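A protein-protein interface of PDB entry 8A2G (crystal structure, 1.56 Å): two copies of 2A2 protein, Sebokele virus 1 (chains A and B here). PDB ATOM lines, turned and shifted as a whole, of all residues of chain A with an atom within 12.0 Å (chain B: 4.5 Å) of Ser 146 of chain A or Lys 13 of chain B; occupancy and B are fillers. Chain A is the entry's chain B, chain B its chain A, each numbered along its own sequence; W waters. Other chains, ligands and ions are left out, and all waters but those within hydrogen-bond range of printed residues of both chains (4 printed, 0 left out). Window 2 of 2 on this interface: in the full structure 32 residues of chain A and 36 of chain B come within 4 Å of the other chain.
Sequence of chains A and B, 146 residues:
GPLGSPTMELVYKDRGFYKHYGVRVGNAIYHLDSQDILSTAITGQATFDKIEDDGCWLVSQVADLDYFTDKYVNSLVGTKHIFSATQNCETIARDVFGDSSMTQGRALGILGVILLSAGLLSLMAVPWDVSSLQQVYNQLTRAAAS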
ATOM      1  N   MET A 124      13.967  -7.452 -12.332  1.00  0.00           N
ATOM      2  CA  MET A 124      15.400  -7.726 -12.245  1.00  0.00           C
ATOM      3  C   MET A 124      16.248  -6.680 -12.949  1.00  0.00           C
ATOM      4  O   MET A 124      17.476  -6.755 -12.876  1.00  0.00           O
ATOM      5  CB  MET A 124      15.679  -9.058 -12.930  1.00  0.00           C
ATOM      6  CG  MET A 124      15.176 -10.164 -12.203  1.00  0.00           C
ATOM      7  SD  MET A 124      15.482 -11.577 -13.275  1.00  0.00           S
ATOM      8  CE  MET A 124      15.082 -12.823 -12.135  1.00  0.00           C
ATOM      9  N   GLN A 135      21.868 -15.045 -19.900  1.00  0.00           N
ATOM     10  CA  GLN A 135      22.494 -15.062 -18.587  1.00  0.00           C
ATOM     11  C   GLN A 135      21.444 -15.278 -17.479  1.00  0.00           C
ATOM     12  O   GLN A 135      21.636 -16.118 -16.591  1.00  0.00           O
ATOM     13  CB  GLN A 135      23.262 -13.758 -18.431  1.00  0.00           C
ATOM     14  CG  GLN A 135      24.187 -13.677 -17.249  1.00  0.00           C
ATOM     15  CD  GLN A 135      25.025 -12.424 -17.347  1.00  0.00           C
ATOM     16  OE1 GLN A 135      24.582 -11.385 -17.846  1.00  0.00           O
ATOM     17  NE2 GLN A 135      26.275 -12.538 -16.931  1.00  0.00           N
ATOM     18  N   VAL A 136      20.325 -14.534 -17.540  1.00  0.00           N
ATOM     19  CA  VAL A 136      19.225 -14.708 -16.595  1.00  0.00           C
ATOM     20  C   VAL A 136      18.656 -16.125 -16.702  1.00  0.00           C
ATOM     21  O   VAL A 136      18.461 -16.794 -15.690  1.00  0.00           O
ATOM     22  CB  VAL A 136      18.140 -13.621 -16.759  1.00  0.00           C
ATOM     23  CG1 VAL A 136      18.638 -12.276 -16.285  1.00  0.00           C
ATOM     24  CG2 VAL A 136      17.595 -13.480 -18.159  1.00  0.00           C
ATOM     25  N   TYR A 137      18.385 -16.587 -17.928  1.00  0.00           N
ATOM     26  CA  TYR A 137      17.809 -17.903 -18.151  1.00  0.00           C
ATOM     27  C   TYR A 137      18.692 -18.997 -17.553  1.00  0.00           C
ATOM     28  O   TYR A 137      18.219 -19.964 -16.964  1.00  0.00           O
ATOM     29  CB  TYR A 137      17.547 -18.156 -19.641  1.00  0.00           C
ATOM     30  CG  TYR A 137      16.838 -19.462 -19.885  1.00  0.00           C
ATOM     31  CD1 TYR A 137      15.485 -19.589 -19.627  1.00  0.00           C
ATOM     32  CD2 TYR A 137      17.529 -20.583 -20.335  1.00  0.00           C
ATOM     33  CE1 TYR A 137      14.824 -20.787 -19.831  1.00  0.00           C
ATOM     34  CE2 TYR A 137      16.871 -21.776 -20.583  1.00  0.00           C
ATOM     35  CZ  TYR A 137      15.518 -21.875 -20.322  1.00  0.00           C
ATOM     36  OH  TYR A 137      14.860 -23.053 -20.548  1.00  0.00           O
ATOM     37  N   ASN A 138      20.002 -18.854 -17.713  1.00  0.00           N
ATOM     38  CA  ASN A 138      20.951 -19.802 -17.139  1.00  0.00           C
ATOM     39  C   ASN A 138      20.827 -19.892 -15.618  1.00  0.00           C
ATOM     40  O   ASN A 138      20.949 -20.984 -15.051  1.00  0.00           O
ATOM     41  CB  ASN A 138      22.386 -19.495 -17.566  1.00  0.00           C
ATOM     42  CG  ASN A 138      22.664 -19.795 -19.022  1.00  0.00           C
ATOM     43  OD1 ASN A 138      21.923 -20.522 -19.682  1.00  0.00           O
ATOM     44  ND2 ASN A 138      23.721 -19.212 -19.553  1.00  0.00           N
ATOM     45  N   GLN A 139      20.640 -18.753 -14.950  1.00  0.00           N
ATOM     46  CA  GLN A 139      20.487 -18.761 -13.502  1.00  0.00           C
ATOM     47  C   GLN A 139      19.136 -19.342 -13.106  1.00  0.00           C
ATOM     48  O   GLN A 139      19.046 -20.064 -12.127  1.00  0.00           O
ATOM     49  CB  GLN A 139      20.646 -17.356 -12.935  1.00  0.00           C
ATOM     50  CG  GLN A 139      22.078 -16.858 -12.977  1.00  0.00           C
ATOM     51  CD  GLN A 139      23.051 -17.785 -12.304  1.00  0.00           C
ATOM     52  OE1 GLN A 139      22.849 -18.193 -11.155  1.00  0.00           O
ATOM     53  NE2 GLN A 139      24.067 -18.192 -13.047  1.00  0.00           N
ATOM     54  N   LEU A 140      18.082 -19.051 -13.862  1.00  0.00           N
ATOM     55  CA  LEU A 140      16.750 -19.555 -13.548  1.00  0.00           C
ATOM     56  C   LEU A 140      16.710 -21.081 -13.645  1.00  0.00           C
ATOM     57  O   LEU A 140      16.004 -21.751 -12.884  1.00  0.00           O
ATOM     58  CB  LEU A 140      15.710 -18.927 -14.477  1.00  0.00           C
ATOM     59  CG  LEU A 140      15.322 -17.476 -14.190  1.00  0.00           C
ATOM     60  CD1 LEU A 140      14.447 -16.899 -15.315  1.00  0.00           C
ATOM     61  CD2 LEU A 140      14.613 -17.344 -12.841  1.00  0.00           C
ATOM     62  N   THR A 141      17.445 -21.654 -14.590  1.00  0.00           N
ATOM     63  CA  THR A 141      17.407 -23.089 -14.832  1.00  0.00           C
ATOM     64  C   THR A 141      18.567 -23.839 -14.162  1.00  0.00           C
ATOM     65  O   THR A 141      18.663 -25.060 -14.284  1.00  0.00           O
ATOM     66  CB  THR A 141      17.305 -23.376 -16.327  1.00  0.00           C
ATOM     67  OG1 THR A 141      18.471 -22.892 -16.986  1.00  0.00           O
ATOM     68  CG2 THR A 141      16.030 -22.788 -16.883  1.00  0.00           C
ATOM     69  N   ARG A 142      19.430 -23.119 -13.429  1.00  0.00           N
ATOM     70  CA  ARG A 142      20.504 -23.740 -12.666  1.00  0.00           C
ATOM     71  C   ARG A 142      19.893 -24.654 -11.591  1.00  0.00           C
ATOM     72  O   ARG A 142      18.818 -24.372 -11.048  1.00  0.00           O
ATOM     73  CB  ARG A 142      21.327 -22.548 -12.142  1.00  0.00           C
ATOM     74  CG  ARG A 142      22.242 -22.769 -10.961  1.00  0.00           C
ATOM     75  CD  ARG A 142      22.895 -21.448 -10.574  1.00  0.00           C
ATOM     76  NE  ARG A 142      23.766 -21.631  -9.423  1.00  0.00           N
ATOM     77  CZ  ARG A 142      24.572 -20.702  -8.897  1.00  0.00           C
ATOM     78  NH1 ARG A 142      24.456 -19.419  -9.226  1.00  0.00           N
ATOM     79  NH2 ARG A 142      25.458 -21.063  -7.983  1.00  0.00           N
ATOM     80  N   ALA A 143      20.562 -25.756 -11.263  1.00  0.00           N
ATOM     81  CA  ALA A 143      20.049 -26.647 -10.226  1.00  0.00           C
ATOM     82  C   ALA A 143      19.816 -25.845  -8.941  1.00  0.00           C
ATOM     83  O   ALA A 143      20.666 -25.082  -8.511  1.00  0.00           O
ATOM     84  CB  ALA A 143      20.979 -27.802  -9.982  1.00  0.00           C
ATOM     85  N   ALA A 144      18.661 -26.041  -8.298  1.00  0.00           N
ATOM     86  CA  ALA A 144      18.260 -25.220  -7.157  1.00  0.00           C
ATOM     87  C   ALA A 144      19.237 -25.337  -5.995  1.00  0.00           C
ATOM     88  O   ALA A 144      19.474 -24.364  -5.284  1.00  0.00           O
ATOM     89  CB  ALA A 144      16.906 -25.649  -6.668  1.00  0.00           C
ATOM     90  N   ALA A 145      19.832 -26.511  -5.778  1.00  0.00           N
ATOM     91  CA  ALA A 145      20.751 -26.675  -4.656  1.00  0.00           C
ATOM     92  C   ALA A 145      22.172 -26.169  -4.966  1.00  0.00           C
ATOM     93  O   ALA A 145      23.016 -26.203  -4.074  1.00  0.00           O
ATOM     94  CB  ALA A 145      20.764 -28.110  -4.250  1.00  0.00           C
ATOM     95  N   SER A 146      22.470 -25.823  -6.228  1.00  0.00           N
ATOM     96  CA  SER A 146      23.825 -25.482  -6.666  1.00  0.00           C
ATOM     97  C   SER A 146      24.229 -24.068  -6.241  1.00  0.00           C
ATOM     98  O   SER A 146      25.368 -23.639  -6.617  1.00  0.00           O
ATOM     99  CB  SER A 146      23.948 -25.674  -8.152  1.00  0.00           C
ATOM    100  OG  SER A 146      23.300 -24.662  -8.886  1.00  0.00           O
ATOM    101  OXT SER A 146      23.439 -23.436  -5.556  1.00  0.00           O
ATOM    102  N   TYR B  12      19.713 -18.389   2.255  1.00  0.00           N
ATOM    103  CA  TYR B  12      19.584 -18.234   0.815  1.00  0.00           C
ATOM    104  C   TYR B  12      20.916 -18.482   0.133  1.00  0.00           C
ATOM    105  O   TYR B  12      21.981 -18.432   0.762  1.00  0.00           O
ATOM    106  CB  TYR B  12      19.086 -16.827   0.478  1.00  0.00           C
ATOM    107  CG  TYR B  12      20.001 -15.707   0.912  1.00  0.00           C
ATOM    108  CD1 TYR B  12      19.904 -15.179   2.170  1.00  0.00           C
ATOM    109  CD2 TYR B  12      20.961 -15.200   0.080  1.00  0.00           C
ATOM    110  CE1 TYR B  12      20.718 -14.147   2.577  1.00  0.00           C
ATOM    111  CE2 TYR B  12      21.805 -14.176   0.467  1.00  0.00           C
ATOM    112  CZ  TYR B  12      21.685 -13.652   1.732  1.00  0.00           C
ATOM    113  OH  TYR B  12      22.483 -12.590   2.191  1.00  0.00           O
ATOM    114  N   LYS B  13      20.835 -18.672  -1.180  1.00  0.00           N
ATOM    115  CA  LYS B  13      21.976 -18.561  -2.065  1.00  0.00           C
ATOM    116  C   LYS B  13      21.679 -17.474  -3.081  1.00  0.00           C
ATOM    117  O   LYS B  13      20.559 -17.330  -3.567  1.00  0.00           O
ATOM    118  CB  LYS B  13      22.249 -19.883  -2.787  1.00  0.00           C
ATOM    119  CG  LYS B  13      22.773 -21.001  -1.901  1.00  0.00           C
ATOM    120  CD  LYS B  13      23.319 -22.170  -2.668  1.00  0.00           C
ATOM    121  CE  LYS B  13      24.010 -23.159  -1.768  1.00  0.00           C
ATOM    122  NZ  LYS B  13      24.576 -24.252  -2.574  1.00  0.00           N
ATOM    123  N   ASP B  14      22.669 -16.615  -3.301  1.00  0.00           N
ATOM    124  CA  ASP B  14      22.519 -15.461  -4.177  1.00  0.00           C
ATOM    125  C   ASP B  14      22.907 -15.802  -5.613  1.00  0.00           C
ATOM    126  O   ASP B  14      24.017 -16.230  -5.880  1.00  0.00           O
ATOM    127  CB  ASP B  14      23.382 -14.330  -3.638  1.00  0.00           C
ATOM    128  CG  ASP B  14      23.114 -12.968  -4.229  1.00  0.00           C
ATOM    129  OD1 ASP B  14      22.432 -12.872  -5.285  1.00  0.00           O
ATOM    130  OD2 ASP B  14      23.561 -11.982  -3.582  1.00  0.00           O
ATOM    131  N   ARG B  15      21.934 -15.684  -6.526  1.00  0.00           N
ATOM    132  CA  ARG B  15      22.141 -15.937  -7.930  1.00  0.00           C
ATOM    133  C   ARG B  15      22.381 -14.643  -8.723  1.00  0.00           C
ATOM    134  O   ARG B  15      22.422 -14.690  -9.954  1.00  0.00           O
ATOM    135  CB  ARG B  15      20.927 -16.657  -8.510  1.00  0.00           C
ATOM    136  CG  ARG B  15      20.378 -17.792  -7.661  1.00  0.00           C
ATOM    137  CD  ARG B  15      21.444 -18.792  -7.380  1.00  0.00           C
ATOM    138  NE  ARG B  15      20.871 -19.996  -6.791  1.00  0.00           N
ATOM    139  CZ  ARG B  15      21.605 -20.968  -6.312  1.00  0.00           C
ATOM    140  NH1 ARG B  15      22.906 -20.790  -6.141  1.00  0.00           N
ATOM    141  NH2 ARG B  15      21.012 -22.132  -6.048  1.00  0.00           N
ATOM    142  N   TYR B  18      18.685 -12.684  -8.489  1.00  0.00           N
ATOM    143  CA  TYR B  18      17.726 -12.914  -7.422  1.00  0.00           C
ATOM    144  C   TYR B  18      18.405 -13.742  -6.342  1.00  0.00           C
ATOM    145  O   TYR B  18      19.472 -14.320  -6.591  1.00  0.00           O
ATOM    146  CB  TYR B  18      16.490 -13.661  -7.957  1.00  0.00           C
ATOM    147  CG  TYR B  18      16.754 -15.037  -8.512  1.00  0.00           C
ATOM    148  CD1 TYR B  18      17.131 -15.219  -9.844  1.00  0.00           C
ATOM    149  CD2 TYR B  18      16.621 -16.166  -7.724  1.00  0.00           C
ATOM    150  CE1 TYR B  18      17.425 -16.476 -10.331  1.00  0.00           C
ATOM    151  CE2 TYR B  18      16.924 -17.432  -8.210  1.00  0.00           C
ATOM    152  CZ  TYR B  18      17.327 -17.588  -9.521  1.00  0.00           C
ATOM    153  OH  TYR B  18      17.609 -18.890  -9.923  1.00  0.00           O
ATOM    154  N   LYS B  19      17.731 -13.874  -5.191  1.00  0.00           N
ATOM    155  CA  LYS B  19      18.171 -14.748  -4.120  1.00  0.00           C
ATOM    156  C   LYS B  19      17.208 -15.924  -4.060  1.00  0.00           C
ATOM    157  O   LYS B  19      15.988 -15.735  -4.108  1.00  0.00           O
ATOM    158  CB  LYS B  19      18.223 -14.019  -2.773  1.00  0.00           C
ATOM    159  CG  LYS B  19      19.359 -13.011  -2.726  1.00  0.00           C
ATOM    160  CD  LYS B  19      19.329 -12.123  -1.502  1.00  0.00           C
ATOM    161  CE  LYS B  19      20.467 -11.137  -1.463  1.00  0.00           C
ATOM    162  NZ  LYS B  19      20.222 -10.127  -0.413  1.00  0.00           N
ATOM    163  N   HIS B  20      17.764 -17.133  -3.909  1.00  0.00           N
ATOM    164  CA  HIS B  20      16.979 -18.346  -3.763  1.00  0.00           C
ATOM    165  C   HIS B  20      16.966 -18.721  -2.279  1.00  0.00           C
ATOM    166  O   HIS B  20      18.005 -19.051  -1.705  1.00  0.00           O
ATOM    167  CB  HIS B  20      17.681 -19.447  -4.559  1.00  0.00           C
ATOM    168  CG  HIS B  20      17.140 -20.827  -4.314  1.00  0.00           C
ATOM    169  ND1 HIS B  20      15.884 -21.196  -4.707  1.00  0.00           N
ATOM    170  CD2 HIS B  20      17.692 -21.907  -3.696  1.00  0.00           C
ATOM    171  CE1 HIS B  20      15.671 -22.459  -4.327  1.00  0.00           C
ATOM    172  NE2 HIS B  20      16.766 -22.923  -3.748  1.00  0.00           N
ATOM    173  N   ASP B  54      25.371 -27.730   2.424  1.00  0.00           N
ATOM    174  CA  ASP B  54      26.716 -27.852   1.862  1.00  0.00           C
ATOM    175  C   ASP B  54      27.673 -26.814   2.451  1.00  0.00           C
ATOM    176  O   ASP B  54      28.881 -26.771   2.099  1.00  0.00           O
ATOM    177  CB  ASP B  54      26.694 -27.716   0.341  1.00  0.00           C
ATOM    178  CG  ASP B  54      26.183 -26.399  -0.205  1.00  0.00           C
ATOM    179  OD1 ASP B  54      25.843 -25.503   0.584  1.00  0.00           O
ATOM    180  OD2 ASP B  54      26.198 -26.224  -1.425  1.00  0.00           O
ATOM    181  N   CYS B  56      27.360 -23.612   2.123  1.00  0.00           N
ATOM    182  CA  CYS B  56      27.430 -22.462   1.242  1.00  0.00           C
ATOM    183  C   CYS B  56      26.139 -21.644   1.178  1.00  0.00           C
ATOM    184  O   CYS B  56      25.929 -20.849   0.258  1.00  0.00           O
ATOM    185  CB  CYS B  56      27.807 -22.933  -0.153  1.00  0.00           C
ATOM    186  SG  CYS B  56      29.471 -23.635  -0.133  1.00  0.00           S
ATOM    187  N   TRP B  57      25.285 -21.744   2.211  1.00  0.00           N
ATOM    188  CA  TRP B  57      24.104 -20.920   2.371  1.00  0.00           C
ATOM    189  C   TRP B  57      24.407 -19.722   3.273  1.00  0.00           C
ATOM    190  O   TRP B  57      25.240 -19.807   4.180  1.00  0.00           O
ATOM    191  CB  TRP B  57      22.970 -21.770   2.927  1.00  0.00           C
ATOM    192  CG  TRP B  57      22.464 -22.842   2.006  1.00  0.00           C
ATOM    193  CD1 TRP B  57      23.018 -24.067   1.801  1.00  0.00           C
ATOM    194  CD2 TRP B  57      21.284 -22.794   1.179  1.00  0.00           C
ATOM    195  NE1 TRP B  57      22.283 -24.774   0.900  1.00  0.00           N
ATOM    196  CE2 TRP B  57      21.236 -24.012   0.457  1.00  0.00           C
ATOM    197  CE3 TRP B  57      20.304 -21.820   0.936  1.00  0.00           C
ATOM    198  CZ2 TRP B  57      20.195 -24.291  -0.427  1.00  0.00           C
ATOM    199  CZ3 TRP B  57      19.284 -22.102   0.043  1.00  0.00           C
ATOM    200  CH2 TRP B  57      19.229 -23.329  -0.622  1.00  0.00           C
HETATM  201  O   HOH W   1      24.753 -18.884  -5.662  1.00  0.00           O
HETATM  202  O   HOH W   2      25.683 -16.874  -7.976  1.00  0.00           O
HETATM  203  O   HOH W   3      26.537 -22.885  -4.169  1.00  0.00           O
HETATM  204  O   HOH W   4      23.827 -28.127  -2.131  1.00  0.00           O
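The side-chain amino group (NZ) of Lys 13 of chain B is in hydrogen-bond range of the backbone carbonyl oxygen (O) of Ala 145 of chain A (2.9 Å). The side-chain amino group of Lys 13 of chain B lies within salt-bridge range of the chain-end carboxylate of Ser 146 of chain A (3.3 Å). NH2 of Arg 15 of chain B lies within hydrogen-bond range of O of Ala 144 of chain A, at 2.8 Å. The chain-end carboxylate of Ser 146 of chain A is in salt-bridge range of the guanidinium group of Arg 15 of chain B (2.8 Å). The side-chain hydroxyl of Tyr 18 of chain B lies within hydrogen-bond range of the backbone carbonyl oxygen of Gln 139 of chain A. NE2 of His 20 of chain B lies close to O of Ala 144 of chain A, 3.4 Å away. NH2 of Arg 142 of chain A lies close to NH1 of Arg 15 of chain B (3.2 Å).
N of His 20 of chain B is in hydrogen-bond range of O of Lys 13 of chain B, at 2.8 Å. The side-chain amino group (NZ) of Lys 13 of chain B lies within salt-bridge range of the side-chain carboxylate (OD2) of Asp 54 of chain B (2.8 Å). The guanidinium group (NH1) of Arg 142 of chain A sits at hydrogen-bond distance from the side-chain amide oxygen (OE1) of Gln 139 of chain A, 2.8 Å away. The chain-end carboxylate (O) of Ser 146 of chain A is in salt-bridge range of the guanidinium group (NH2) of Arg 142 of chain A. The side-chain hydroxyl (OG) of Ser 146 of chain A is in hydrogen-bond range of the backbone carbonyl oxygen (O) of Ala 143 of chain A (2.7 Å).
Among the printed residues, merely in contact across the chains: Gln 139 of chain A with Arg 15 of chain B (3.6 Å), Leu 140 of chain A with Tyr 18 of chain B (3.8 Å), Ala 143 of chain A with Arg 15 of chain B (3.9 Å) and Met 124 of chain A with Tyr 18 of chain B (3.9 Å).
Val 136 of chain A touches none of the printed residues of chain B. Asn 138 of chain A touches none of the printed residues of chain B. Of the printed residues of chain B, Leu 140 of chain A touches Tyr 18 (3.8 Å). Of the printed residues of chain B, Arg 142 of chain A touches Arg 15 (3.2 Å). Printed residues of chain B within 4 Å of Ala 144 of chain A: Arg 15 and His 20. Of the printed residues of chain B, Ser 146 of chain A touches Lys 13 (3.2 Å) and Arg 15 (2.8 Å). No residue of chain A comes within 4 Å of Tyr 12 of chain B. Of chain A, only Ala 145 (2.9 Å) and Ser 146 (3.2 Å) come within 4 Å of Lys 13 of chain B. No residue of chain A comes within 4 Å of Asp 14 of chain B. Of chain A, only Met 124 (3.9 Å), Gln 139 (2.9 Å) and Leu 140 (3.8 Å) come within 4 Å of Tyr 18 of chain B. No residue of chain A comes within 4 Å of Lys 19 of chain B. His 20 of chain B touches one residue of chain A. Asp 54 of chain B touches none of the printed residues of chain A. No residue of chain A comes within 4 Å of Cys 56 of chain B. The nearest residue of chain A that does not touch Lys 13 of chain B is Ala 144 of chain A (5.1 Å). The nearest printed residue of chain B that does not touch Leu 140 of chain A is Arg 15 of chain B (6.5 Å).
Of the 10 printed residues of chain B, 4 touch a printed residue of chain A. Among the printed residues, 11 pairs touch across the chains. Among the printed residues, no Asp or Glu carboxylate lies within 4 Å of a Lys or Arg side-chain nitrogen of the other chain.
No position is printed for both chains. Of the 11 pairs that touch across the chains among the printed residues, none has its exchanged pair printed and touching as well.
Water W1 lies within hydrogen-bond range of NH1 of Arg 15 of chain B (2.7 Å), O of Asp 14 of chain B (2.8 Å) and NH2 of Arg 142 of chain A (3.3 Å). Water W2 bridges O of Asp 14 of chain B (2.8 Å) and NH1 of Arg 142 of chain A (3.1 Å). Water W3 lies within hydrogen-bond range of the chain-end carboxylate (O) of Ser 146 of chain A (2.8 Å) and the side-chain amino group (NZ) of Lys 13 of chain B (2.9 Å). Water W4 bridges the backbone carbonyl oxygen (O) of Ala 145 of chain A and the side-chain carboxylate (OD2) of Asp 54 of chain B.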
